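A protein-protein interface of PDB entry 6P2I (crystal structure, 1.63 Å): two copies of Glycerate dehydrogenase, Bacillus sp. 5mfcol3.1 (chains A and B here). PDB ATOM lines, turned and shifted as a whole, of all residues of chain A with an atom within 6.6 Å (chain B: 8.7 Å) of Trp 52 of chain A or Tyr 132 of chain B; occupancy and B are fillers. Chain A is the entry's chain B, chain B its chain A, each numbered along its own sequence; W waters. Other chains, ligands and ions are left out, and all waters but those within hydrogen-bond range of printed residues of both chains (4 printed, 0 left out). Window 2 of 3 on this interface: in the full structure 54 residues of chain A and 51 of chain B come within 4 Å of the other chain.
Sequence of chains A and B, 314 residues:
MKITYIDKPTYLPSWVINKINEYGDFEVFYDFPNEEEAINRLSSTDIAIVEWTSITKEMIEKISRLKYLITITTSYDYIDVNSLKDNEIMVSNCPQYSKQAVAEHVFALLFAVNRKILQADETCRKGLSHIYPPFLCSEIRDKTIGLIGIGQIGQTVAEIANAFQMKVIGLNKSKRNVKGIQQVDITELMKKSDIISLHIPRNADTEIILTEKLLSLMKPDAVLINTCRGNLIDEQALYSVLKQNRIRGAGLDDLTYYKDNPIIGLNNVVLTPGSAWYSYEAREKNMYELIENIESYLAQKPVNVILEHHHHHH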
ATOM      1  N   TYR A   5      28.099  15.915  16.108  1.00  0.00           N
ATOM      2  CA  TYR A   5      27.372  16.810  15.208  1.00  0.00           C
ATOM      3  C   TYR A   5      26.229  17.396  16.032  1.00  0.00           C
ATOM      4  O   TYR A   5      25.277  16.691  16.375  1.00  0.00           O
ATOM      5  CB  TYR A   5      26.875  16.033  13.989  1.00  0.00           C
ATOM      6  CG  TYR A   5      26.603  16.817  12.711  1.00  0.00           C
ATOM      7  CD1 TYR A   5      25.785  17.941  12.706  1.00  0.00           C
ATOM      8  CD2 TYR A   5      27.131  16.390  11.494  1.00  0.00           C
ATOM      9  CE1 TYR A   5      25.511  18.640  11.509  1.00  0.00           C
ATOM     10  CE2 TYR A   5      26.862  17.082  10.294  1.00  0.00           C
ATOM     11  CZ  TYR A   5      26.058  18.208  10.321  1.00  0.00           C
ATOM     12  OH  TYR A   5      25.773  18.892   9.145  1.00  0.00           O
ATOM     13  N   ASP A   7      23.849  19.754  15.826  1.00  0.00           N
ATOM     14  CA  ASP A   7      22.509  20.091  15.372  1.00  0.00           C
ATOM     15  C   ASP A   7      22.195  19.269  14.130  1.00  0.00           C
ATOM     16  O   ASP A   7      23.058  18.577  13.589  1.00  0.00           O
ATOM     17  CB  ASP A   7      22.354  21.594  15.104  1.00  0.00           C
ATOM     18  CG  ASP A   7      23.525  22.191  14.351  1.00  0.00           C
ATOM     19  OD1 ASP A   7      24.222  21.459  13.616  1.00  0.00           O
ATOM     20  OD2 ASP A   7      23.744  23.414  14.495  1.00  0.00           O
ATOM     21  N   LYS A   8      20.944  19.350  13.684  1.00  0.00           N
ATOM     22  CA  LYS A   8      20.412  18.410  12.701  1.00  0.00           C
ATOM     23  C   LYS A   8      21.154  18.485  11.372  1.00  0.00           C
ATOM     24  O   LYS A   8      21.124  19.531  10.708  1.00  0.00           O
ATOM     25  CB  LYS A   8      18.927  18.659  12.462  1.00  0.00           C
ATOM     26  CG  LYS A   8      18.324  17.659  11.489  1.00  0.00           C
ATOM     27  CD  LYS A   8      16.906  18.029  11.111  1.00  0.00           C
ATOM     28  CE  LYS A   8      15.977  17.865  12.293  1.00  0.00           C
ATOM     29  NZ  LYS A   8      14.550  18.086  11.915  1.00  0.00           N
ATOM     30  N   PRO A   9      21.812  17.414  10.943  1.00  0.00           N
ATOM     31  CA  PRO A   9      22.493  17.447   9.647  1.00  0.00           C
ATOM     32  C   PRO A   9      21.492  17.404   8.509  1.00  0.00           C
ATOM     33  O   PRO A   9      20.515  16.651   8.544  1.00  0.00           O
ATOM     34  CB  PRO A   9      23.372  16.191   9.671  1.00  0.00           C
ATOM     35  CG  PRO A   9      22.725  15.286  10.654  1.00  0.00           C
ATOM     36  CD  PRO A   9      22.013  16.144  11.659  1.00  0.00           C
ATOM     37  N   THR A  10      21.729  18.243   7.498  1.00  0.00           N
ATOM     38  CA  THR A  10      20.957  18.119   6.267  1.00  0.00           C
ATOM     39  C   THR A  10      21.261  16.796   5.576  1.00  0.00           C
ATOM     40  O   THR A  10      20.360  16.153   5.023  1.00  0.00           O
ATOM     41  CB  THR A  10      21.251  19.302   5.337  1.00  0.00           C
ATOM     42  OG1 THR A  10      20.695  20.500   5.903  1.00  0.00           O
ATOM     43  CG2 THR A  10      20.626  19.066   3.958  1.00  0.00           C
ATOM     44  N   ASP A  31      18.217  17.543  15.900  1.00  0.00           N
ATOM     45  CA  ASP A  31      17.346  18.575  16.448  1.00  0.00           C
ATOM     46  C   ASP A  31      18.037  19.924  16.284  1.00  0.00           C
ATOM     47  O   ASP A  31      19.068  20.037  15.613  1.00  0.00           O
ATOM     48  CB  ASP A  31      17.007  18.271  17.914  1.00  0.00           C
ATOM     49  CG  ASP A  31      18.244  18.130  18.790  1.00  0.00           C
ATOM     50  OD1 ASP A  31      18.105  17.689  19.946  1.00  0.00           O
ATOM     51  OD2 ASP A  31      19.356  18.465  18.335  1.00  0.00           O
ATOM     52  N   PHE A  32      17.483  20.952  16.915  1.00  0.00           N
ATOM     53  CA  PHE A  32      18.107  22.275  16.915  1.00  0.00           C
ATOM     54  C   PHE A  32      18.311  22.740  18.345  1.00  0.00           C
ATOM     55  O   PHE A  32      17.326  23.098  19.020  1.00  0.00           O
ATOM     56  CB  PHE A  32      17.252  23.276  16.141  1.00  0.00           C
ATOM     57  CG  PHE A  32      17.047  22.900  14.710  1.00  0.00           C
ATOM     58  CD1 PHE A  32      18.085  23.016  13.800  1.00  0.00           C
ATOM     59  CD2 PHE A  32      15.829  22.407  14.276  1.00  0.00           C
ATOM     60  CE1 PHE A  32      17.911  22.660  12.481  1.00  0.00           C
ATOM     61  CE2 PHE A  32      15.645  22.048  12.955  1.00  0.00           C
ATOM     62  CZ  PHE A  32      16.685  22.174  12.056  1.00  0.00           C
ATOM     63  N   PRO A  33      19.540  22.755  18.860  1.00  0.00           N
ATOM     64  CA  PRO A  33      19.744  23.087  20.273  1.00  0.00           C
ATOM     65  C   PRO A  33      19.597  24.575  20.540  1.00  0.00           C
ATOM     66  O   PRO A  33      19.877  25.420  19.687  1.00  0.00           O
ATOM     67  CB  PRO A  33      21.184  22.630  20.534  1.00  0.00           C
ATOM     68  CG  PRO A  33      21.856  22.815  19.204  1.00  0.00           C
ATOM     69  CD  PRO A  33      20.808  22.439  18.181  1.00  0.00           C
ATOM     70  N   VAL A  50      29.077  21.646  13.344  1.00  0.00           N
ATOM     71  CA  VAL A  50      27.928  22.534  13.504  1.00  0.00           C
ATOM     72  C   VAL A  50      27.404  22.924  12.132  1.00  0.00           C
ATOM     73  O   VAL A  50      28.184  23.103  11.190  1.00  0.00           O
ATOM     74  CB  VAL A  50      28.284  23.788  14.332  1.00  0.00           C
ATOM     75  CG1 VAL A  50      29.379  24.609  13.651  1.00  0.00           C
ATOM     76  CG2 VAL A  50      27.031  24.642  14.591  1.00  0.00           C
ATOM     77  N   GLU A  51      26.076  23.044  12.018  1.00  0.00           N
ATOM     78  CA  GLU A  51      25.440  23.447  10.769  1.00  0.00           C
ATOM     79  C   GLU A  51      24.554  24.673  10.906  1.00  0.00           C
ATOM     80  O   GLU A  51      24.536  25.516  10.005  1.00  0.00           O
ATOM     81  CB  GLU A  51      24.598  22.293  10.193  1.00  0.00           C
ATOM     82  CG  GLU A  51      23.811  22.712   8.950  1.00  0.00           C
ATOM     83  CD  GLU A  51      23.315  21.540   8.126  1.00  0.00           C
ATOM     84  OE1 GLU A  51      23.645  20.387   8.458  1.00  0.00           O
ATOM     85  OE2 GLU A  51      22.597  21.785   7.134  1.00  0.00           O
ATOM     86  N   TRP A  52      23.815  24.792  12.003  1.00  0.00           N
ATOM     87  CA  TRP A  52      22.779  25.805  12.141  1.00  0.00           C
ATOM     88  C   TRP A  52      23.009  26.779  13.277  1.00  0.00           C
ATOM     89  O   TRP A  52      22.506  27.904  13.221  1.00  0.00           O
ATOM     90  CB  TRP A  52      21.415  25.139  12.376  1.00  0.00           C
ATOM     91  CG  TRP A  52      21.025  24.145  11.335  1.00  0.00           C
ATOM     92  CD1 TRP A  52      21.201  22.792  11.378  1.00  0.00           C
ATOM     93  CD2 TRP A  52      20.371  24.431  10.102  1.00  0.00           C
ATOM     94  NE1 TRP A  52      20.703  22.217  10.233  1.00  0.00           N
ATOM     95  CE2 TRP A  52      20.187  23.203   9.434  1.00  0.00           C
ATOM     96  CE3 TRP A  52      19.927  25.606   9.492  1.00  0.00           C
ATOM     97  CZ2 TRP A  52      19.569  23.120   8.185  1.00  0.00           C
ATOM     98  CZ3 TRP A  52      19.318  25.520   8.246  1.00  0.00           C
ATOM     99  CH2 TRP A  52      19.145  24.288   7.611  1.00  0.00           C
ATOM    100  N   THR A  53      23.743  26.377  14.306  1.00  0.00           N
ATOM    101  CA  THR A  53      23.685  27.032  15.602  1.00  0.00           C
ATOM    102  C   THR A  53      24.719  28.142  15.702  1.00  0.00           C
ATOM    103  O   THR A  53      25.907  27.921  15.454  1.00  0.00           O
ATOM    104  CB  THR A  53      23.905  26.002  16.708  1.00  0.00           C
ATOM    105  OG1 THR A  53      22.974  24.925  16.532  1.00  0.00           O
ATOM    106  CG2 THR A  53      23.720  26.633  18.083  1.00  0.00           C
ATOM    107  N   SER A  54      24.262  29.332  16.079  1.00  0.00           N
ATOM    108  CA  SER A  54      25.181  30.422  16.366  1.00  0.00           C
ATOM    109  C   SER A  54      26.064  30.059  17.553  1.00  0.00           C
ATOM    110  O   SER A  54      25.596  29.503  18.549  1.00  0.00           O
ATOM    111  CB  SER A  54      24.399  31.704  16.656  1.00  0.00           C
ATOM    112  OG  SER A  54      23.948  32.299  15.448  1.00  0.00           O
ATOM    113  N   ILE A  72      30.021  22.727   8.873  1.00  0.00           N
ATOM    114  CA  ILE A  72      29.730  21.972   7.663  1.00  0.00           C
ATOM    115  C   ILE A  72      29.541  22.903   6.480  1.00  0.00           C
ATOM    116  O   ILE A  72      29.575  22.463   5.321  1.00  0.00           O
ATOM    117  CB  ILE A  72      28.478  21.101   7.904  1.00  0.00           C
ATOM    118  CG1 ILE A  72      28.430  19.919   6.932  1.00  0.00           C
ATOM    119  CG2 ILE A  72      27.215  21.953   7.780  1.00  0.00           C
ATOM    120  CD1 ILE A  72      29.587  18.932   7.118  1.00  0.00           C
ATOM    121  N   THR A  73      29.365  24.188   6.759  1.00  0.00           N
ATOM    122  CA  THR A  73      29.148  25.227   5.769  1.00  0.00           C
ATOM    123  C   THR A  73      30.472  25.841   5.320  1.00  0.00           C
ATOM    124  O   THR A  73      31.502  25.729   5.988  1.00  0.00           O
ATOM    125  CB  THR A  73      28.252  26.322   6.352  1.00  0.00           C
ATOM    126  OG1 THR A  73      28.884  26.875   7.511  1.00  0.00           O
ATOM    127  CG2 THR A  73      26.899  25.753   6.766  1.00  0.00           C
ATOM    128  N   TYR A  78      28.322  33.033  11.431  1.00  0.00           N
ATOM    129  CA  TYR A  78      27.571  32.812  12.659  1.00  0.00           C
ATOM    130  C   TYR A  78      28.435  32.255  13.780  1.00  0.00           C
ATOM    131  O   TYR A  78      27.925  31.999  14.874  1.00  0.00           O
ATOM    132  CB  TYR A  78      26.393  31.868  12.392  1.00  0.00           C
ATOM    133  CG  TYR A  78      26.771  30.495  11.852  1.00  0.00           C
ATOM    134  CD1 TYR A  78      27.262  30.333  10.559  1.00  0.00           C
ATOM    135  CD2 TYR A  78      26.611  29.356  12.635  1.00  0.00           C
ATOM    136  CE1 TYR A  78      27.588  29.076  10.068  1.00  0.00           C
ATOM    137  CE2 TYR A  78      26.933  28.102  12.156  1.00  0.00           C
ATOM    138  CZ  TYR A  78      27.424  27.963  10.875  1.00  0.00           C
ATOM    139  OH  TYR A  78      27.744  26.706  10.402  1.00  0.00           O
ATOM    140  N   PRO A 273      14.879  29.458  -1.647  1.00  0.00           N
ATOM    141  CA  PRO A 273      15.002  29.447  -0.182  1.00  0.00           C
ATOM    142  C   PRO A 273      16.356  28.908   0.287  1.00  0.00           C
ATOM    143  O   PRO A 273      16.431  27.939   1.050  1.00  0.00           O
ATOM    144  CB  PRO A 273      13.845  28.539   0.240  1.00  0.00           C
ATOM    145  CG  PRO A 273      13.789  27.521  -0.869  1.00  0.00           C
ATOM    146  CD  PRO A 273      14.140  28.274  -2.142  1.00  0.00           C
ATOM    147  N   GLY A 274      17.429  29.552  -0.159  1.00  0.00           N
ATOM    148  CA  GLY A 274      18.741  29.093   0.283  1.00  0.00           C
ATOM    149  C   GLY A 274      19.146  27.771  -0.319  1.00  0.00           C
ATOM    150  O   GLY A 274      20.011  27.089   0.225  1.00  0.00           O
ATOM    151  N   SER A 275      18.546  27.398  -1.444  1.00  0.00           N
ATOM    152  CA  SER A 275      18.711  26.089  -2.059  1.00  0.00           C
ATOM    153  C   SER A 275      19.798  26.056  -3.122  1.00  0.00           C
ATOM    154  O   SER A 275      19.988  25.014  -3.751  1.00  0.00           O
ATOM    155  CB  SER A 275      17.380  25.646  -2.680  1.00  0.00           C
ATOM    156  OG  SER A 275      16.895  26.655  -3.559  1.00  0.00           O
ATOM    157  N   ALA A 276      20.526  27.159  -3.319  1.00  0.00           N
ATOM    158  CA  ALA A 276      21.536  27.230  -4.375  1.00  0.00           C
ATOM    159  C   ALA A 276      22.556  26.102  -4.281  1.00  0.00           C
ATOM    160  O   ALA A 276      23.020  25.581  -5.302  1.00  0.00           O
ATOM    161  CB  ALA A 276      22.261  28.577  -4.310  1.00  0.00           C
ATOM    162  N   TRP A 277      22.933  25.729  -3.064  1.00  0.00           N
ATOM    163  CA  TRP A 277      24.027  24.788  -2.865  1.00  0.00           C
ATOM    164  C   TRP A 277      23.639  23.332  -3.057  1.00  0.00           C
ATOM    165  O   TRP A 277      24.526  22.484  -3.165  1.00  0.00           O
ATOM    166  CB  TRP A 277      24.571  24.927  -1.447  1.00  0.00           C
ATOM    167  CG  TRP A 277      23.653  24.358  -0.391  1.00  0.00           C
ATOM    168  CD1 TRP A 277      22.533  24.946   0.134  1.00  0.00           C
ATOM    169  CD2 TRP A 277      23.794  23.094   0.282  1.00  0.00           C
ATOM    170  NE1 TRP A 277      21.982  24.136   1.102  1.00  0.00           N
ATOM    171  CE2 TRP A 277      22.728  22.990   1.207  1.00  0.00           C
ATOM    172  CE3 TRP A 277      24.727  22.049   0.206  1.00  0.00           C
ATOM    173  CZ2 TRP A 277      22.570  21.883   2.051  1.00  0.00           C
ATOM    174  CZ3 TRP A 277      24.562  20.945   1.042  1.00  0.00           C
ATOM    175  CH2 TRP A 277      23.496  20.875   1.959  1.00  0.00           C
ATOM    176  N   TYR A 278      22.348  23.000  -3.059  1.00  0.00           N
ATOM    177  CA  TYR A 278      21.952  21.645  -2.673  1.00  0.00           C
ATOM    178  C   TYR A 278      21.840  20.725  -3.888  1.00  0.00           C
ATOM    179  O   TYR A 278      20.760  20.300  -4.299  1.00  0.00           O
ATOM    180  CB  TYR A 278      20.662  21.671  -1.867  1.00  0.00           C
ATOM    181  CG  TYR A 278      20.462  20.403  -1.059  1.00  0.00           C
ATOM    182  CD1 TYR A 278      21.541  19.781  -0.442  1.00  0.00           C
ATOM    183  CD2 TYR A 278      19.213  19.813  -0.933  1.00  0.00           C
ATOM    184  CE1 TYR A 278      21.381  18.623   0.292  1.00  0.00           C
ATOM    185  CE2 TYR A 278      19.043  18.645  -0.188  1.00  0.00           C
ATOM    186  CZ  TYR A 278      20.137  18.056   0.417  1.00  0.00           C
ATOM    187  OH  TYR A 278      20.012  16.896   1.162  1.00  0.00           O
ATOM    188  N   ARG B 115      16.172  23.028 -10.777  1.00  0.00           N
ATOM    189  CA  ARG B 115      16.174  23.718  -9.496  1.00  0.00           C
ATOM    190  C   ARG B 115      14.766  23.913  -8.951  1.00  0.00           C
ATOM    191  O   ARG B 115      14.610  24.503  -7.875  1.00  0.00           O
ATOM    192  CB  ARG B 115      16.887  25.081  -9.630  1.00  0.00           C
ATOM    193  CG  ARG B 115      18.338  25.038 -10.146  1.00  0.00           C
ATOM    194  CD  ARG B 115      19.132  24.080  -9.297  1.00  0.00           C
ATOM    195  NE  ARG B 115      20.550  23.945  -9.629  1.00  0.00           N
ATOM    196  CZ  ARG B 115      21.551  24.374  -8.850  1.00  0.00           C
ATOM    197  NH1 ARG B 115      21.302  25.056  -7.751  1.00  0.00           N
ATOM    198  NH2 ARG B 115      22.808  24.133  -9.184  1.00  0.00           N
ATOM    199  N   LYS B 116      13.743  23.431  -9.669  1.00  0.00           N
ATOM    200  CA  LYS B 116      12.343  23.568  -9.265  1.00  0.00           C
ATOM    201  C   LYS B 116      12.027  25.014  -8.915  1.00  0.00           C
ATOM    202  O   LYS B 116      11.440  25.318  -7.874  1.00  0.00           O
ATOM    203  CB  LYS B 116      12.002  22.627  -8.106  1.00  0.00           C
ATOM    204  CG  LYS B 116      12.075  21.150  -8.468  1.00  0.00           C
ATOM    205  CD  LYS B 116      11.595  20.257  -7.320  1.00  0.00           C
ATOM    206  CE  LYS B 116      11.682  18.785  -7.698  1.00  0.00           C
ATOM    207  NZ  LYS B 116      13.091  18.316  -7.845  1.00  0.00           N
ATOM    208  N   THR B 123       7.690  28.729  -2.357  1.00  0.00           N
ATOM    209  CA  THR B 123       8.104  28.492  -0.977  1.00  0.00           C
ATOM    210  C   THR B 123       8.465  29.795  -0.276  1.00  0.00           C
ATOM    211  O   THR B 123       8.011  30.063   0.844  1.00  0.00           O
ATOM    212  CB  THR B 123       9.298  27.531  -0.973  1.00  0.00           C
ATOM    213  OG1 THR B 123       8.889  26.264  -1.507  1.00  0.00           O
ATOM    214  CG2 THR B 123       9.874  27.350   0.439  1.00  0.00           C
ATOM    215  N   SER B 129      12.049  29.665   4.575  1.00  0.00           N
ATOM    216  CA  SER B 129      13.433  29.927   4.219  1.00  0.00           C
ATOM    217  C   SER B 129      14.298  28.740   4.616  1.00  0.00           C
ATOM    218  O   SER B 129      13.937  27.941   5.487  1.00  0.00           O
ATOM    219  CB  SER B 129      13.944  31.214   4.880  1.00  0.00           C
ATOM    220  OG  SER B 129      13.861  31.145   6.294  1.00  0.00           O
ATOM    221  N   HIS B 130      15.454  28.645   3.955  1.00  0.00           N
ATOM    222  CA  HIS B 130      16.441  27.590   4.200  1.00  0.00           C
ATOM    223  C   HIS B 130      15.793  26.212   4.103  1.00  0.00           C
ATOM    224  O   HIS B 130      15.898  25.374   5.005  1.00  0.00           O
ATOM    225  CB  HIS B 130      17.140  27.802   5.542  1.00  0.00           C
ATOM    226  CG  HIS B 130      17.871  29.105   5.623  1.00  0.00           C
ATOM    227  ND1 HIS B 130      19.087  29.311   5.008  1.00  0.00           N
ATOM    228  CD2 HIS B 130      17.539  30.280   6.206  1.00  0.00           C
ATOM    229  CE1 HIS B 130      19.485  30.551   5.231  1.00  0.00           C
ATOM    230  NE2 HIS B 130      18.563  31.160   5.953  1.00  0.00           N
ATOM    231  N   ILE B 131      15.116  25.992   2.975  1.00  0.00           N
ATOM    232  CA  ILE B 131      14.386  24.766   2.682  1.00  0.00           C
ATOM    233  C   ILE B 131      15.182  24.004   1.634  1.00  0.00           C
ATOM    234  O   ILE B 131      15.287  24.440   0.480  1.00  0.00           O
ATOM    235  CB  ILE B 131      12.964  25.065   2.182  1.00  0.00           C
ATOM    236  CG1 ILE B 131      12.201  25.924   3.202  1.00  0.00           C
ATOM    237  CG2 ILE B 131      12.243  23.777   1.850  1.00  0.00           C
ATOM    238  CD1 ILE B 131      11.943  25.254   4.550  1.00  0.00           C
ATOM    239  N   TYR B 132      15.747  22.867   2.020  1.00  0.00           N
ATOM    240  CA  TYR B 132      16.644  22.176   1.100  1.00  0.00           C
ATOM    241  C   TYR B 132      16.074  20.882   0.517  1.00  0.00           C
ATOM    242  O   TYR B 132      16.181  20.686  -0.700  1.00  0.00           O
ATOM    243  CB  TYR B 132      17.983  21.867   1.786  1.00  0.00           C
ATOM    244  CG  TYR B 132      18.622  23.032   2.508  1.00  0.00           C
ATOM    245  CD1 TYR B 132      18.518  24.330   2.016  1.00  0.00           C
ATOM    246  CD2 TYR B 132      19.343  22.832   3.674  1.00  0.00           C
ATOM    247  CE1 TYR B 132      19.106  25.397   2.681  1.00  0.00           C
ATOM    248  CE2 TYR B 132      19.934  23.891   4.346  1.00  0.00           C
ATOM    249  CZ  TYR B 132      19.814  25.167   3.842  1.00  0.00           C
ATOM    250  OH  TYR B 132      20.401  26.215   4.516  1.00  0.00           O
ATOM    251  N   PRO B 133      15.492  19.980   1.318  1.00  0.00           N
ATOM    252  CA  PRO B 133      15.133  18.632   0.806  1.00  0.00           C
ATOM    253  C   PRO B 133      14.306  18.660  -0.472  1.00  0.00           C
ATOM    254  O   PRO B 133      14.606  17.896  -1.403  1.00  0.00           O
ATOM    255  CB  PRO B 133      14.347  18.012   1.971  1.00  0.00           C
ATOM    256  CG  PRO B 133      14.957  18.633   3.173  1.00  0.00           C
ATOM    257  CD  PRO B 133      15.275  20.052   2.782  1.00  0.00           C
ATOM    258  N   PRO B 134      13.266  19.504  -0.589  1.00  0.00           N
ATOM    259  CA  PRO B 134      12.481  19.481  -1.836  1.00  0.00           C
ATOM    260  C   PRO B 134      13.257  19.934  -3.057  1.00  0.00           C
ATOM    261  O   PRO B 134      12.806  19.677  -4.183  1.00  0.00           O
ATOM    262  CB  PRO B 134      11.310  20.436  -1.548  1.00  0.00           C
ATOM    263  CG  PRO B 134      11.280  20.593  -0.071  1.00  0.00           C
ATOM    264  CD  PRO B 134      12.719  20.504   0.347  1.00  0.00           C
ATOM    265  N   PHE B 135      14.417  20.570  -2.878  1.00  0.00           N
ATOM    266  CA  PHE B 135      15.139  21.219  -3.966  1.00  0.00           C
ATOM    267  C   PHE B 135      16.497  20.583  -4.224  1.00  0.00           C
ATOM    268  O   PHE B 135      17.324  21.161  -4.934  1.00  0.00           O
ATOM    269  CB  PHE B 135      15.251  22.712  -3.662  1.00  0.00           C
ATOM    270  CG  PHE B 135      13.911  23.334  -3.444  1.00  0.00           C
ATOM    271  CD1 PHE B 135      13.035  23.451  -4.511  1.00  0.00           C
ATOM    272  CD2 PHE B 135      13.488  23.716  -2.188  1.00  0.00           C
ATOM    273  CE1 PHE B 135      11.765  23.972  -4.334  1.00  0.00           C
ATOM    274  CE2 PHE B 135      12.217  24.249  -2.000  1.00  0.00           C
ATOM    275  CZ  PHE B 135      11.353  24.375  -3.078  1.00  0.00           C
ATOM    276  N   LEU B 136      16.722  19.393  -3.678  1.00  0.00           N
ATOM    277  CA  LEU B 136      17.886  18.592  -4.046  1.00  0.00           C
ATOM    278  C   LEU B 136      17.960  18.450  -5.556  1.00  0.00           C
ATOM    279  O   LEU B 136      17.023  17.944  -6.185  1.00  0.00           O
ATOM    280  CB  LEU B 136      17.787  17.217  -3.400  1.00  0.00           C
ATOM    281  CG  LEU B 136      18.901  16.219  -3.702  1.00  0.00           C
ATOM    282  CD1 LEU B 136      20.245  16.754  -3.202  1.00  0.00           C
ATOM    283  CD2 LEU B 136      18.571  14.899  -3.051  1.00  0.00           C
ATOM    284  N   CYS B 137      19.067  18.899  -6.140  1.00  0.00           N
ATOM    285  CA  CYS B 137      19.184  18.980  -7.587  1.00  0.00           C
ATOM    286  C   CYS B 137      20.442  18.263  -8.055  1.00  0.00           C
ATOM    287  O   CYS B 137      21.260  17.787  -7.258  1.00  0.00           O
ATOM    288  CB  CYS B 137      19.208  20.438  -8.064  1.00  0.00           C
ATOM    289  SG  CYS B 137      20.743  21.298  -7.650  1.00  0.00           S
HETATM  290  O   HOH W   1      16.202  31.080   2.554  1.00  0.00           O
HETATM  291  O   HOH W   2      16.574  25.460  -6.020  1.00  0.00           O
HETATM  292  O   HOH W   3      18.475  23.551  -5.685  1.00  0.00           O
HETATM  293  O   HOH W   4      22.421  24.597   6.428  1.00  0.00           O
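Of chain B, only Tyr 132 (3.4 Å) comes within 4 Å of Trp 52 of chain A. Of the printed residues of chain A, Tyr 132 of chain B touches Thr 10, Trp 52, Gly 274, Trp 277 and Tyr 278. Printed residues of chain B within 4 Å of Pro 273 of chain A: His 130 (3.1 Å), Ile 131 (3.0 Å) and Phe 135 (3.8 Å). Printed residues of chain B within 4 Å of Thr 10 of chain A: Tyr 132 (3.5 Å). Printed residues of chain A within 4 Å of Leu 136 of chain B: Tyr 278 (3.4 Å).
Printed residues of chain B that touch a printed residue of chain A: Arg 115, His 130, Ile 131, Tyr 132, Phe 135, Leu 136 and Cys 137. Hydrophobic or aromatic side chains of chain A within 4 Å of the printed part of chain B: Trp 52, Pro 273, Trp 277 and Tyr 278. Among the printed residues, 14 pairs touch across the chains.
No position is printed for both chains.
The backbone carbonyl oxygen (O) of Lys 8 of chain A is in hydrogen-bond range of the indole nitrogen (NE1) of Trp 52 of chain A (2.8 Å). A ring nitrogen (ND1) of His 130 of chain B lies within hydrogen-bond range of the side-chain hydroxyl (OH) of Tyr 132 of chain B, at 3.4 Å. The side-chain carboxylate of Glu 51 of chain A is in hydrogen-bond range of the side-chain hydroxyl of Thr 10 of chain A. The side-chain carboxylate (OD2) of Asp 7 of chain A is in hydrogen-bond range of the backbone NH (N) of Trp 52 of chain A. The side-chain sulfur of Cys 137 of chain B is in hydrogen-bond range of the guanidinium group of Arg 115 of chain B, at 3.3 Å.
The backbone carbonyl oxygen (O) of Tyr 278 of chain A lies within hydrogen-bond range of the backbone NH (N) of Cys 137 of chain B, at 2.9 Å. The guanidinium group (NH1) of Arg 115 of chain B sits at hydrogen-bond distance from the backbone carbonyl oxygen (O) of Ala 276 of chain A (3.0 Å). The backbone carbonyl oxygen of Pro 273 of chain A lies within hydrogen-bond range of the backbone NH of His 130 of chain B, at 3.1 Å. N of Ile 131 of chain B lies within hydrogen-bond range of O of Pro 273 of chain A (3.0 Å).
Water W2 bridges the side-chain hydroxyl of Ser 275 of chain A (2.8 Å) and the backbone carbonyl oxygen of Arg 115 of chain B (2.9 Å). Water W3 lies within hydrogen-bond range of O of Phe 135 of chain B (2.8 Å), O of Ser 275 of chain A (2.9 Å) and SG of Cys 137 of chain B (3.8 Å). Water W4 bridges the side-chain carboxylate (OE2) of Glu 51 of chain A (2.9 Å) and the side-chain hydroxyl (OH) of Tyr 132 of chain B (3.2 Å). Water W1 lies within hydrogen-bond range of N of His 130 of chain B (2.9 Å), N of Gly 274 of chain A (3.3 Å) and O of Pro 273 of chain A (3.5 Å).
Among the printed residues, merely in contact across the chains: Thr 10 of chain A with Tyr 132 of chain B, Trp 52 of chain A with Tyr 132 of chain B, Pro 273 of chain A with Phe 135 of chain B, Gly 274 of chain A with Tyr 132 of chain B, Ser 275 of chain A with Ile 131 of chain B, Ser 275 of chain A with Phe 135 of chain B, Trp 277 of chain A with Tyr 132 of chain B, Tyr 278 of chain A with Tyr 132 of chain B, Tyr 278 of chain A with Phe 135 of chain B and Tyr 278 of chain A with Leu 136 of chain B.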
